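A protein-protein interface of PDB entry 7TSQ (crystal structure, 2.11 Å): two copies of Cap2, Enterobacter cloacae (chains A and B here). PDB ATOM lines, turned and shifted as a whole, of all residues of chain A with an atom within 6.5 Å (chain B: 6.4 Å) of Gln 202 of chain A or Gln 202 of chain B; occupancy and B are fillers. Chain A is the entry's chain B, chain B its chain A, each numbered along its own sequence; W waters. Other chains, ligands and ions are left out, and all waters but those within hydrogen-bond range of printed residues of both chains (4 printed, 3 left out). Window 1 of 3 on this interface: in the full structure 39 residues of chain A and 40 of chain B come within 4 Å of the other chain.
Asn 37 of chain A touches Gln 202 of chain B, and with the chains exchanged Gln 202 of chain A touches Asn 37 of chain B.
Arg 40 of chain A touches Ala 198 of chain B, and with the chains exchanged Ala 198 of chain A touches Arg 40 of chain B.
Asp 199 of chain A touches Ala 206 of chain B, and with the chains exchanged Ala 206 of chain A touches Asp 199 of chain B.
Leu 203 of chain A touches Val 207 of chain B, and with the chains exchanged Val 207 of chain A touches Leu 203 of chain B.
18 positions are printed for both chains.
Water W3 bridges OD1 of Asn 37 of chain A (2.7 Å) and NE2 of Gln 202 of chain B (3.1 Å).
Water W4 lies within hydrogen-bond range of the side-chain amide oxygen (OD1) of Asn 37 of chain B (2.7 Å), the side-chain amide nitrogen (NE2) of Gln 202 of chain A (3.1 Å) and the side-chain carboxylate (OE2) of Glu 36 of chain B (3.4 Å).
Water W2 lies within hydrogen-bond range of N of Ala 198 of chain B (2.8 Å) and O of Arg 40 of chain A (3.2 Å).
Among the printed residues, merely in contact across the chains: Ala 206 of chain A with Asp 199 of chain B (3.4 Å), Asp 199 of chain A with Ala 206 of chain B (3.5 Å), Leu 203 of chain A with Leu 203 of chain B (3.6 Å), Arg 40 of chain A with Ala 198 of chain B (3.6 Å), Ala 198 of chain A with Arg 40 of chain B (3.6 Å), Asn 37 of chain A with Gln 202 of chain B (3.7 Å), Leu 203 of chain A with Ala 206 of chain B (3.7 Å), Ala 206 of chain A with Leu 203 of chain B (3.7 Å), Gln 202 of chain A with Asn 37 of chain B (3.8 Å), Leu 203 of chain A with Val 207 of chain B (3.8 Å) and Val 207 of chain A with Leu 203 of chain B (3.9 Å).
NH2 of Arg 197 of chain B lies within salt-bridge range of OD2 of Asp 199 of chain B.
The guanidinium group of Arg 40 of chain A lies within salt-bridge range of the side-chain carboxylate of Glu 36 of chain A, at 2.9 Å.
ND2 of Asn 37 of chain B is in hydrogen-bond range of O of Ala 205 of chain B (3.3 Å).
The side-chain carboxylate (OE2) of Glu 36 of chain B lies within salt-bridge range of the guanidinium group (NH2) of Arg 40 of chain B, at 3.0 Å.
Printed residues of chain A that touch a printed residue of chain B: Asn 37, Arg 40, His 62, Ala 63, Ala 198, Asp 199, Gln 202, Leu 203, Ala 206 and Val 207.
Hydrophobic or aromatic side chains of chain A that line the printed part of chain B: Ala 198, Leu 203, Ala 206 and Val 207.
Of the 18 printed residues of chain B, 10 touch a printed residue of chain A.
Printed residues of chain B that touch a printed residue of chain A: Asn 37, Arg 40, His 62, Ala 63, Ala 198, Asp 199, Gln 202, Leu 203, Ala 206 and Val 207.
Hydrophobic or aromatic side chains of chain B within 4 Å of the printed part of chain A: Ala 198, Leu 203, Ala 206 and Val 207.
OE1 of Gln 202 of chain B sits close to OE1 of Gln 202 of chain A, at 3.1 Å.
The guanidinium group (NE) of Arg 40 of chain B sits close to the backbone carbonyl oxygen (O) of His 62 of chain A (3.1 Å).
NH2 of Arg 40 of chain B lies within hydrogen-bond range of O of Ala 63 of chain A (3.4 Å).
O of Ala 63 of chain B lies within hydrogen-bond range of NH2 of Arg 40 of chain A, at 3.5 Å.
The guanidinium group of Arg 40 of chain A lies close to the backbone carbonyl oxygen of His 62 of chain B, 3.0 Å away.
Of the printed residues of chain B, Asn 37 of chain A touches Gln 202.
Of the printed residues of chain B, Arg 40 of chain A touches His 62 (2.9 Å), Ala 63 (3.5 Å) and Ala 198 (3.6 Å).
Of chain B, only Asn 37 and Gln 202 come within 4 Å of Gln 202 of chain A.
Ala 205 of chain A touches none of the printed residues of chain B.
Of the printed residues of chain A, Asp 199 of chain B touches Ala 206 (3.4 Å).
Gln 202 of chain B touches just these residues of chain A: Asn 37 and Gln 202.
The nearest residue of chain B that does not touch Gln 202 of chain A is Ala 206 of chain B (4.4 Å).
The nearest printed residue of chain B that does not touch Asp 199 of chain A is Asn 37 of chain B (4.5 Å).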
ATOM      1  N   LEU A  30      -6.443  22.306  -0.549  1.00  0.00           N
ATOM      2  CA  LEU A  30      -6.329  23.713  -0.204  1.00  0.00           C
ATOM      3  C   LEU A  30      -6.285  23.939   1.301  1.00  0.00           C
ATOM      4  O   LEU A  30      -5.553  24.806   1.797  1.00  0.00           O
ATOM      5  CB  LEU A  30      -7.492  24.501  -0.817  1.00  0.00           C
ATOM      6  CG  LEU A  30      -7.513  26.036  -0.736  1.00  0.00           C
ATOM      7  CD1 LEU A  30      -6.341  26.629  -1.509  1.00  0.00           C
ATOM      8  CD2 LEU A  30      -8.839  26.603  -1.251  1.00  0.00           C
ATOM      9  N   MET A  33      -2.766  23.025   3.030  1.00  0.00           N
ATOM     10  CA  MET A  33      -1.740  24.028   2.769  1.00  0.00           C
ATOM     11  C   MET A  33      -2.040  25.330   3.490  1.00  0.00           C
ATOM     12  O   MET A  33      -1.145  25.960   4.054  1.00  0.00           O
ATOM     13  CB  MET A  33      -1.611  24.263   1.265  1.00  0.00           C
ATOM     14  CG  MET A  33      -1.158  23.028   0.484  1.00  0.00           C
ATOM     15  SD  MET A  33      -1.025  23.330  -1.294  1.00  0.00           S
ATOM     16  CE  MET A  33      -1.004  21.663  -1.941  1.00  0.00           C
ATOM     17  N   GLU A  36      -1.125  24.904   7.139  1.00  0.00           N
ATOM     18  CA  GLU A  36       0.316  24.979   7.356  1.00  0.00           C
ATOM     19  C   GLU A  36       0.809  26.417   7.279  1.00  0.00           C
ATOM     20  O   GLU A  36       1.580  26.874   8.129  1.00  0.00           O
ATOM     21  CB  GLU A  36       1.063  24.094   6.351  1.00  0.00           C
ATOM     22  CG  GLU A  36       2.580  24.073   6.590  1.00  0.00           C
ATOM     23  CD  GLU A  36       3.342  23.068   5.730  1.00  0.00           C
ATOM     24  OE1 GLU A  36       2.705  22.342   4.937  1.00  0.00           O
ATOM     25  OE2 GLU A  36       4.586  23.009   5.856  1.00  0.00           O
ATOM     26  N   ASN A  37       0.370  27.165   6.249  1.00  0.00           N
ATOM     27  CA  ASN A  37       0.741  28.574   6.150  1.00  0.00           C
ATOM     28  C   ASN A  37       0.394  29.322   7.421  1.00  0.00           C
ATOM     29  O   ASN A  37       1.215  30.057   7.975  1.00  0.00           O
ATOM     30  CB  ASN A  37       0.045  29.243   4.966  1.00  0.00           C
ATOM     31  CG  ASN A  37       0.630  28.845   3.633  1.00  0.00           C
ATOM     32  OD1 ASN A  37       1.522  28.022   3.555  1.00  0.00           O
ATOM     33  ND2 ASN A  37       0.096  29.410   2.570  1.00  0.00           N
ATOM     34  N   ARG A  40       2.661  28.521  10.361  1.00  0.00           N
ATOM     35  CA  ARG A  40       3.993  29.099  10.247  1.00  0.00           C
ATOM     36  C   ARG A  40       4.021  30.603  10.472  1.00  0.00           C
ATOM     37  O   ARG A  40       5.060  31.129  10.881  1.00  0.00           O
ATOM     38  CB  ARG A  40       4.603  28.750   8.884  1.00  0.00           C
ATOM     39  CG  ARG A  40       4.984  27.250   8.773  1.00  0.00           C
ATOM     40  CD  ARG A  40       5.798  26.890   7.519  1.00  0.00           C
ATOM     41  NE  ARG A  40       5.916  25.444   7.349  1.00  0.00           N
ATOM     42  CZ  ARG A  40       6.847  24.687   7.921  1.00  0.00           C
ATOM     43  NH1 ARG A  40       7.776  25.206   8.705  1.00  0.00           N
ATOM     44  NH2 ARG A  40       6.832  23.374   7.701  1.00  0.00           N
ATOM     45  N   HIS A  62      -1.050  18.223  -1.904  1.00  0.00           N
ATOM     46  CA  HIS A  62      -1.337  18.144  -0.475  1.00  0.00           C
ATOM     47  C   HIS A  62      -0.096  18.572   0.297  1.00  0.00           C
ATOM     48  O   HIS A  62       1.011  18.642  -0.246  1.00  0.00           O
ATOM     49  CB  HIS A  62      -1.749  16.724  -0.061  1.00  0.00           C
ATOM     50  CG  HIS A  62      -2.666  16.675   1.125  1.00  0.00           C
ATOM     51  ND1 HIS A  62      -2.206  16.551   2.422  1.00  0.00           N
ATOM     52  CD2 HIS A  62      -4.019  16.715   1.209  1.00  0.00           C
ATOM     53  CE1 HIS A  62      -3.235  16.534   3.249  1.00  0.00           C
ATOM     54  NE2 HIS A  62      -4.345  16.634   2.542  1.00  0.00           N
ATOM     55  N   ALA A  63      -0.291  18.872   1.583  1.00  0.00           N
ATOM     56  CA  ALA A  63       0.811  19.272   2.452  1.00  0.00           C
ATOM     57  C   ALA A  63       1.536  18.104   3.102  1.00  0.00           C
ATOM     58  O   ALA A  63       2.700  18.261   3.495  1.00  0.00           O
ATOM     59  CB  ALA A  63       0.307  20.209   3.549  1.00  0.00           C
ATOM     60  N   ARG A 197      -2.142  21.034 -10.388  1.00  0.00           N
ATOM     61  CA  ARG A 197      -0.875  20.526  -9.883  1.00  0.00           C
ATOM     62  C   ARG A 197      -0.554  21.172  -8.540  1.00  0.00           C
ATOM     63  O   ARG A 197      -1.286  22.031  -8.038  1.00  0.00           O
ATOM     64  CB  ARG A 197       0.270  20.780 -10.872  1.00  0.00           C
ATOM     65  CG  ARG A 197       0.112  20.116 -12.247  1.00  0.00           C
ATOM     66  CD  ARG A 197       1.420  20.148 -13.063  1.00  0.00           C
ATOM     67  NE  ARG A 197       1.930  21.503 -13.271  1.00  0.00           N
ATOM     68  CZ  ARG A 197       3.066  21.791 -13.892  1.00  0.00           C
ATOM     69  NH1 ARG A 197       3.840  20.844 -14.397  1.00  0.00           N
ATOM     70  NH2 ARG A 197       3.437  23.066 -14.008  1.00  0.00           N
ATOM     71  N   ALA A 198       0.575  20.760  -7.947  1.00  0.00           N
ATOM     72  CA  ALA A 198       0.965  21.290  -6.645  1.00  0.00           C
ATOM     73  C   ALA A 198       1.261  22.779  -6.704  1.00  0.00           C
ATOM     74  O   ALA A 198       1.037  23.501  -5.723  1.00  0.00           O
ATOM     75  CB  ALA A 198       2.187  20.549  -6.104  1.00  0.00           C
ATOM     76  N   ASP A 199       1.776  23.267  -7.834  1.00  0.00           N
ATOM     77  CA  ASP A 199       2.038  24.698  -7.941  1.00  0.00           C
ATOM     78  C   ASP A 199       0.765  25.507  -8.170  1.00  0.00           C
ATOM     79  O   ASP A 199       0.730  26.698  -7.834  1.00  0.00           O
ATOM     80  CB  ASP A 199       3.075  24.994  -9.042  1.00  0.00           C
ATOM     81  CG  ASP A 199       2.714  24.404 -10.401  1.00  0.00           C
ATOM     82  OD1 ASP A 199       1.706  23.678 -10.505  1.00  0.00           O
ATOM     83  OD2 ASP A 199       3.471  24.669 -11.364  1.00  0.00           O
ATOM     84  N   ASP A 200      -0.289  24.889  -8.716  1.00  0.00           N
ATOM     85  CA  ASP A 200      -1.574  25.570  -8.820  1.00  0.00           C
ATOM     86  C   ASP A 200      -2.242  25.738  -7.461  1.00  0.00           C
ATOM     87  O   ASP A 200      -2.787  26.799  -7.148  1.00  0.00           O
ATOM     88  CB  ASP A 200      -2.524  24.814  -9.750  1.00  0.00           C
ATOM     89  CG  ASP A 200      -1.971  24.618 -11.151  1.00  0.00           C
ATOM     90  OD1 ASP A 200      -1.657  25.624 -11.822  1.00  0.00           O
ATOM     91  OD2 ASP A 200      -1.843  23.445 -11.577  1.00  0.00           O
ATOM     92  N   VAL A 201      -2.249  24.681  -6.642  1.00  0.00           N
ATOM     93  CA  VAL A 201      -2.907  24.743  -5.345  1.00  0.00           C
ATOM     94  C   VAL A 201      -2.087  25.542  -4.337  1.00  0.00           C
ATOM     95  O   VAL A 201      -2.641  26.262  -3.503  1.00  0.00           O
ATOM     96  CB  VAL A 201      -3.183  23.318  -4.828  1.00  0.00           C
ATOM     97  CG1 VAL A 201      -3.906  23.364  -3.489  1.00  0.00           C
ATOM     98  CG2 VAL A 201      -3.973  22.510  -5.840  1.00  0.00           C
ATOM     99  N   GLN A 202      -0.749  25.440  -4.387  1.00  0.00           N
ATOM    100  CA  GLN A 202       0.071  26.217  -3.463  1.00  0.00           C
ATOM    101  C   GLN A 202      -0.090  27.714  -3.701  1.00  0.00           C
ATOM    102  O   GLN A 202      -0.165  28.501  -2.754  1.00  0.00           O
ATOM    103  CB  GLN A 202       1.542  25.824  -3.562  1.00  0.00           C
ATOM    104  CG  GLN A 202       1.910  24.494  -2.891  1.00  0.00           C
ATOM    105  CD  GLN A 202       2.046  24.573  -1.373  1.00  0.00           C
ATOM    106  OE1 GLN A 202       1.765  25.599  -0.757  1.00  0.00           O
ATOM    107  NE2 GLN A 202       2.478  23.474  -0.762  1.00  0.00           N
ATOM    108  N   LEU A 203      -0.146  28.133  -4.974  1.00  0.00           N
ATOM    109  CA  LEU A 203      -0.400  29.536  -5.276  1.00  0.00           C
ATOM    110  C   LEU A 203      -1.698  30.007  -4.643  1.00  0.00           C
ATOM    111  O   LEU A 203      -1.745  31.046  -3.977  1.00  0.00           O
ATOM    112  CB  LEU A 203      -0.440  29.753  -6.791  1.00  0.00           C
ATOM    113  CG  LEU A 203      -0.540  31.203  -7.283  1.00  0.00           C
ATOM    114  CD1 LEU A 203       0.816  31.907  -7.203  1.00  0.00           C
ATOM    115  CD2 LEU A 203      -1.089  31.304  -8.702  1.00  0.00           C
ATOM    116  N   TRP A 204      -2.782  29.250  -4.829  1.00  0.00           N
ATOM    117  CA  TRP A 204      -4.056  29.666  -4.258  1.00  0.00           C
ATOM    118  C   TRP A 204      -4.054  29.571  -2.741  1.00  0.00           C
ATOM    119  O   TRP A 204      -4.711  30.380  -2.079  1.00  0.00           O
ATOM    120  CB  TRP A 204      -5.198  28.825  -4.833  1.00  0.00           C
ATOM    121  CG  TRP A 204      -5.638  29.185  -6.269  1.00  0.00           C
ATOM    122  CD1 TRP A 204      -6.046  28.310  -7.234  1.00  0.00           C
ATOM    123  CD2 TRP A 204      -5.716  30.495  -6.868  1.00  0.00           C
ATOM    124  NE1 TRP A 204      -6.376  28.984  -8.388  1.00  0.00           N
ATOM    125  CE2 TRP A 204      -6.180  30.324  -8.191  1.00  0.00           C
ATOM    126  CE3 TRP A 204      -5.442  31.788  -6.417  1.00  0.00           C
ATOM    127  CZ2 TRP A 204      -6.375  31.399  -9.059  1.00  0.00           C
ATOM    128  CZ3 TRP A 204      -5.630  32.849  -7.276  1.00  0.00           C
ATOM    129  CH2 TRP A 204      -6.095  32.651  -8.583  1.00  0.00           C
ATOM    130  N   ALA A 205      -3.303  28.624  -2.157  1.00  0.00           N
ATOM    131  CA  ALA A 205      -3.161  28.585  -0.703  1.00  0.00           C
ATOM    132  C   ALA A 205      -2.538  29.869  -0.180  1.00  0.00           C
ATOM    133  O   ALA A 205      -2.997  30.452   0.805  1.00  0.00           O
ATOM    134  CB  ALA A 205      -2.329  27.381  -0.269  1.00  0.00           C
ATOM    135  N   ALA A 206      -1.481  30.337  -0.849  1.00  0.00           N
ATOM    136  CA  ALA A 206      -0.858  31.598  -0.473  1.00  0.00           C
ATOM    137  C   ALA A 206      -1.830  32.760  -0.623  1.00  0.00           C
ATOM    138  O   ALA A 206      -1.990  33.577   0.282  1.00  0.00           O
ATOM    139  CB  ALA A 206       0.394  31.841  -1.314  1.00  0.00           C
ATOM    140  N   VAL A 207      -2.482  32.865  -1.787  1.00  0.00           N
ATOM    141  CA  VAL A 207      -3.467  33.925  -1.993  1.00  0.00           C
ATOM    142  C   VAL A 207      -4.529  33.885  -0.913  1.00  0.00           C
ATOM    143  O   VAL A 207      -4.920  34.916  -0.358  1.00  0.00           O
ATOM    144  CB  VAL A 207      -4.087  33.811  -3.399  1.00  0.00           C
ATOM    145  CG1 VAL A 207      -5.245  34.790  -3.554  1.00  0.00           C
ATOM    146  CG2 VAL A 207      -3.018  34.057  -4.447  1.00  0.00           C
ATOM    147  N   LEU B  30      13.038  29.421  -0.159  1.00  0.00           N
ATOM    148  CA  LEU B  30      12.493  29.265  -1.503  1.00  0.00           C
ATOM    149  C   LEU B  30      12.876  27.926  -2.112  1.00  0.00           C
ATOM    150  O   LEU B  30      12.039  27.252  -2.722  1.00  0.00           O
ATOM    151  CB  LEU B  30      12.964  30.411  -2.398  1.00  0.00           C
ATOM    152  CG  LEU B  30      12.404  30.558  -3.814  1.00  0.00           C
ATOM    153  CD1 LEU B  30      10.946  30.982  -3.748  1.00  0.00           C
ATOM    154  CD2 LEU B  30      13.216  31.552  -4.629  1.00  0.00           C
ATOM    155  N   MET B  33      10.762  24.844  -0.808  1.00  0.00           N
ATOM    156  CA  MET B  33       9.384  24.814  -1.278  1.00  0.00           C
ATOM    157  C   MET B  33       9.303  24.522  -2.770  1.00  0.00           C
ATOM    158  O   MET B  33       8.378  23.851  -3.228  1.00  0.00           O
ATOM    159  CB  MET B  33       8.692  26.134  -0.956  1.00  0.00           C
ATOM    160  CG  MET B  33       8.551  26.422   0.541  1.00  0.00           C
ATOM    161  SD  MET B  33       7.691  27.978   0.899  1.00  0.00           S
ATOM    162  CE  MET B  33       7.948  28.160   2.662  1.00  0.00           C
ATOM    163  N   GLU B  36       9.931  20.738  -3.160  1.00  0.00           N
ATOM    164  CA  GLU B  36       8.718  19.988  -2.853  1.00  0.00           C
ATOM    165  C   GLU B  36       7.718  20.073  -3.994  1.00  0.00           C
ATOM    166  O   GLU B  36       7.147  19.067  -4.414  1.00  0.00           O
ATOM    167  CB  GLU B  36       8.098  20.506  -1.557  1.00  0.00           C
ATOM    168  CG  GLU B  36       6.885  19.719  -1.076  1.00  0.00           C
ATOM    169  CD  GLU B  36       6.222  20.338   0.148  1.00  0.00           C
ATOM    170  OE1 GLU B  36       6.874  21.137   0.856  1.00  0.00           O
ATOM    171  OE2 GLU B  36       5.036  20.033   0.397  1.00  0.00           O
ATOM    172  N   ASN B  37       7.483  21.286  -4.522  1.00  0.00           N
ATOM    173  CA  ASN B  37       6.576  21.438  -5.653  1.00  0.00           C
ATOM    174  C   ASN B  37       6.990  20.547  -6.812  1.00  0.00           C
ATOM    175  O   ASN B  37       6.167  19.844  -7.403  1.00  0.00           O
ATOM    176  CB  ASN B  37       6.526  22.895  -6.112  1.00  0.00           C
ATOM    177  CG  ASN B  37       5.839  23.806  -5.116  1.00  0.00           C
ATOM    178  OD1 ASN B  37       5.361  23.375  -4.079  1.00  0.00           O
ATOM    179  ND2 ASN B  37       5.808  25.086  -5.430  1.00  0.00           N
ATOM    180  N   ARG B  40       6.265  16.869  -6.191  1.00  0.00           N
ATOM    181  CA  ARG B  40       4.851  16.520  -6.263  1.00  0.00           C
ATOM    182  C   ARG B  40       4.356  16.473  -7.698  1.00  0.00           C
ATOM    183  O   ARG B  40       3.444  15.699  -8.008  1.00  0.00           O
ATOM    184  CB  ARG B  40       4.029  17.501  -5.417  1.00  0.00           C
ATOM    185  CG  ARG B  40       4.291  17.335  -3.898  1.00  0.00           C
ATOM    186  CD  ARG B  40       3.300  18.097  -3.004  1.00  0.00           C
ATOM    187  NE  ARG B  40       3.733  18.103  -1.607  1.00  0.00           N
ATOM    188  CZ  ARG B  40       3.523  17.107  -0.754  1.00  0.00           C
ATOM    189  NH1 ARG B  40       2.897  16.002  -1.119  1.00  0.00           N
ATOM    190  NH2 ARG B  40       3.956  17.226   0.500  1.00  0.00           N
ATOM    191  N   HIS B  62       9.760  27.768   5.746  1.00  0.00           N
ATOM    192  CA  HIS B  62      10.477  26.590   5.255  1.00  0.00           C
ATOM    193  C   HIS B  62       9.485  25.455   5.025  1.00  0.00           C
ATOM    194  O   HIS B  62       8.371  25.464   5.548  1.00  0.00           O
ATOM    195  CB  HIS B  62      11.570  26.140   6.240  1.00  0.00           C
ATOM    196  CG  HIS B  62      12.805  25.596   5.586  1.00  0.00           C
ATOM    197  ND1 HIS B  62      12.933  24.279   5.194  1.00  0.00           N
ATOM    198  CD2 HIS B  62      13.981  26.196   5.272  1.00  0.00           C
ATOM    199  CE1 HIS B  62      14.127  24.098   4.657  1.00  0.00           C
ATOM    200  NE2 HIS B  62      14.779  25.246   4.684  1.00  0.00           N
ATOM    201  N   ALA B  63       9.916  24.468   4.238  1.00  0.00           N
ATOM    202  CA  ALA B  63       9.105  23.272   4.020  1.00  0.00           C
ATOM    203  C   ALA B  63       9.241  22.231   5.127  1.00  0.00           C
ATOM    204  O   ALA B  63       8.339  21.400   5.292  1.00  0.00           O
ATOM    205  CB  ALA B  63       9.469  22.632   2.686  1.00  0.00           C
ATOM    206  N   ARG B 197       6.798  36.296   5.068  1.00  0.00           N
ATOM    207  CA  ARG B 197       6.154  35.250   5.855  1.00  0.00           C
ATOM    208  C   ARG B 197       6.106  33.971   5.028  1.00  0.00           C
ATOM    209  O   ARG B 197       6.560  33.936   3.884  1.00  0.00           O
ATOM    210  CB  ARG B 197       4.747  35.673   6.295  1.00  0.00           C
ATOM    211  CG  ARG B 197       4.691  37.018   7.022  1.00  0.00           C
ATOM    212  CD  ARG B 197       3.291  37.320   7.559  1.00  0.00           C
ATOM    213  NE  ARG B 197       2.271  37.272   6.515  1.00  0.00           N
ATOM    214  CZ  ARG B 197       0.974  37.441   6.724  1.00  0.00           C
ATOM    215  NH1 ARG B 197       0.494  37.693   7.931  1.00  0.00           N
ATOM    216  NH2 ARG B 197       0.132  37.349   5.695  1.00  0.00           N
ATOM    217  N   ALA B 198       5.545  32.909   5.615  1.00  0.00           N
ATOM    218  CA  ALA B 198       5.427  31.645   4.896  1.00  0.00           C
ATOM    219  C   ALA B 198       4.654  31.804   3.601  1.00  0.00           C
ATOM    220  O   ALA B 198       5.056  31.295   2.550  1.00  0.00           O
ATOM    221  CB  ALA B 198       4.761  30.593   5.773  1.00  0.00           C
ATOM    222  N   ASP B 199       3.545  32.559   3.638  1.00  0.00           N
ATOM    223  CA  ASP B 199       2.714  32.656   2.445  1.00  0.00           C
ATOM    224  C   ASP B 199       3.398  33.449   1.341  1.00  0.00           C
ATOM    225  O   ASP B 199       3.224  33.120   0.158  1.00  0.00           O
ATOM    226  CB  ASP B 199       1.328  33.228   2.763  1.00  0.00           C
ATOM    227  CG  ASP B 199       1.352  34.582   3.464  1.00  0.00           C
ATOM    228  OD1 ASP B 199       2.436  35.069   3.846  1.00  0.00           O
ATOM    229  OD2 ASP B 199       0.251  35.163   3.632  1.00  0.00           O
ATOM    230  N   ASP B 200       4.233  34.440   1.683  1.00  0.00           N
ATOM    231  CA  ASP B 200       5.000  35.155   0.673  1.00  0.00           C
ATOM    232  C   ASP B 200       5.959  34.224  -0.052  1.00  0.00           C
ATOM    233  O   ASP B 200       6.062  34.247  -1.281  1.00  0.00           O
ATOM    234  CB  ASP B 200       5.781  36.309   1.294  1.00  0.00           C
ATOM    235  CG  ASP B 200       4.888  37.400   1.875  1.00  0.00           C
ATOM    236  OD1 ASP B 200       4.210  38.125   1.111  1.00  0.00           O
ATOM    237  OD2 ASP B 200       4.866  37.532   3.117  1.00  0.00           O
ATOM    238  N   VAL B 201       6.694  33.396   0.704  1.00  0.00           N
ATOM    239  CA  VAL B 201       7.657  32.493   0.091  1.00  0.00           C
ATOM    240  C   VAL B 201       6.947  31.393  -0.674  1.00  0.00           C
ATOM    241  O   VAL B 201       7.414  30.932  -1.721  1.00  0.00           O
ATOM    242  CB  VAL B 201       8.607  31.912   1.156  1.00  0.00           C
ATOM    243  CG1 VAL B 201       9.620  30.966   0.509  1.00  0.00           C
ATOM    244  CG2 VAL B 201       9.313  33.024   1.905  1.00  0.00           C
ATOM    245  N   GLN B 202       5.782  30.954  -0.176  1.00  0.00           N
ATOM    246  CA  GLN B 202       5.013  29.939  -0.887  1.00  0.00           C
ATOM    247  C   GLN B 202       4.473  30.485  -2.194  1.00  0.00           C
ATOM    248  O   GLN B 202       4.355  29.772  -3.197  1.00  0.00           O
ATOM    249  CB  GLN B 202       3.871  29.409  -0.005  1.00  0.00           C
ATOM    250  CG  GLN B 202       4.279  28.496   1.156  1.00  0.00           C
ATOM    251  CD  GLN B 202       4.569  27.059   0.734  1.00  0.00           C
ATOM    252  OE1 GLN B 202       4.650  26.748  -0.448  1.00  0.00           O
ATOM    253  NE2 GLN B 202       4.748  26.182   1.714  1.00  0.00           N
ATOM    254  N   LEU B 203       4.093  31.769  -2.195  1.00  0.00           N
ATOM    255  CA  LEU B 203       3.617  32.376  -3.425  1.00  0.00           C
ATOM    256  C   LEU B 203       4.720  32.414  -4.466  1.00  0.00           C
ATOM    257  O   LEU B 203       4.503  32.074  -5.633  1.00  0.00           O
ATOM    258  CB  LEU B 203       3.095  33.789  -3.170  1.00  0.00           C
ATOM    259  CG  LEU B 203       2.310  34.460  -4.311  1.00  0.00           C
ATOM    260  CD1 LEU B 203       0.845  34.019  -4.321  1.00  0.00           C
ATOM    261  CD2 LEU B 203       2.418  35.974  -4.227  1.00  0.00           C
ATOM    262  N   TRP B 204       5.923  32.816  -4.064  1.00  0.00           N
ATOM    263  CA  TRP B 204       7.023  32.893  -5.013  1.00  0.00           C
ATOM    264  C   TRP B 204       7.645  31.536  -5.328  1.00  0.00           C
ATOM    265  O   TRP B 204       8.347  31.410  -6.342  1.00  0.00           O
ATOM    266  CB  TRP B 204       8.104  33.847  -4.490  1.00  0.00           C
ATOM    267  CG  TRP B 204       7.703  35.344  -4.480  1.00  0.00           C
ATOM    268  CD1 TRP B 204       7.975  36.261  -3.503  1.00  0.00           C
ATOM    269  CD2 TRP B 204       6.977  36.063  -5.496  1.00  0.00           C
ATOM    270  NE1 TRP B 204       7.464  37.491  -3.841  1.00  0.00           N
ATOM    271  CE2 TRP B 204       6.848  37.398  -5.059  1.00  0.00           C
ATOM    272  CE3 TRP B 204       6.426  35.707  -6.728  1.00  0.00           C
ATOM    273  CZ2 TRP B 204       6.195  38.374  -5.814  1.00  0.00           C
ATOM    274  CZ3 TRP B 204       5.773  36.676  -7.472  1.00  0.00           C
ATOM    275  CH2 TRP B 204       5.661  37.991  -7.014  1.00  0.00           C
ATOM    276  N   ALA B 205       7.436  30.525  -4.482  1.00  0.00           N
ATOM    277  CA  ALA B 205       7.818  29.165  -4.847  1.00  0.00           C
ATOM    278  C   ALA B 205       6.877  28.561  -5.879  1.00  0.00           C
ATOM    279  O   ALA B 205       7.310  27.778  -6.733  1.00  0.00           O
ATOM    280  CB  ALA B 205       7.845  28.263  -3.617  1.00  0.00           C
ATOM    281  N   ALA B 206       5.593  28.921  -5.826  1.00  0.00           N
ATOM    282  CA  ALA B 206       4.657  28.498  -6.855  1.00  0.00           C
ATOM    283  C   ALA B 206       4.923  29.202  -8.176  1.00  0.00           C
ATOM    284  O   ALA B 206       4.854  28.589  -9.242  1.00  0.00           O
ATOM    285  CB  ALA B 206       3.230  28.751  -6.387  1.00  0.00           C
ATOM    286  N   VAL B 207       5.223  30.506  -8.135  1.00  0.00           N
ATOM    287  CA  VAL B 207       5.500  31.230  -9.369  1.00  0.00           C
ATOM    288  C   VAL B 207       6.813  30.786  -9.991  1.00  0.00           C
ATOM    289  O   VAL B 207       6.955  30.745 -11.219  1.00  0.00           O
ATOM    290  CB  VAL B 207       5.494  32.745  -9.103  1.00  0.00           C
ATOM    291  CG1 VAL B 207       5.992  33.504 -10.324  1.00  0.00           C
ATOM    292  CG2 VAL B 207       4.089  33.210  -8.717  1.00  0.00           C
HETATM  293  O   HOH W   1       1.304  18.076  -8.491  1.00  0.00           O
HETATM  294  O   HOH W   2       5.781  33.042   8.362  1.00  0.00           O
HETATM  295  O   HOH W   3       3.708  26.879   4.584  1.00  0.00           O
HETATM  296  O   HOH W   4       4.147  21.534  -2.544  1.00  0.00           O
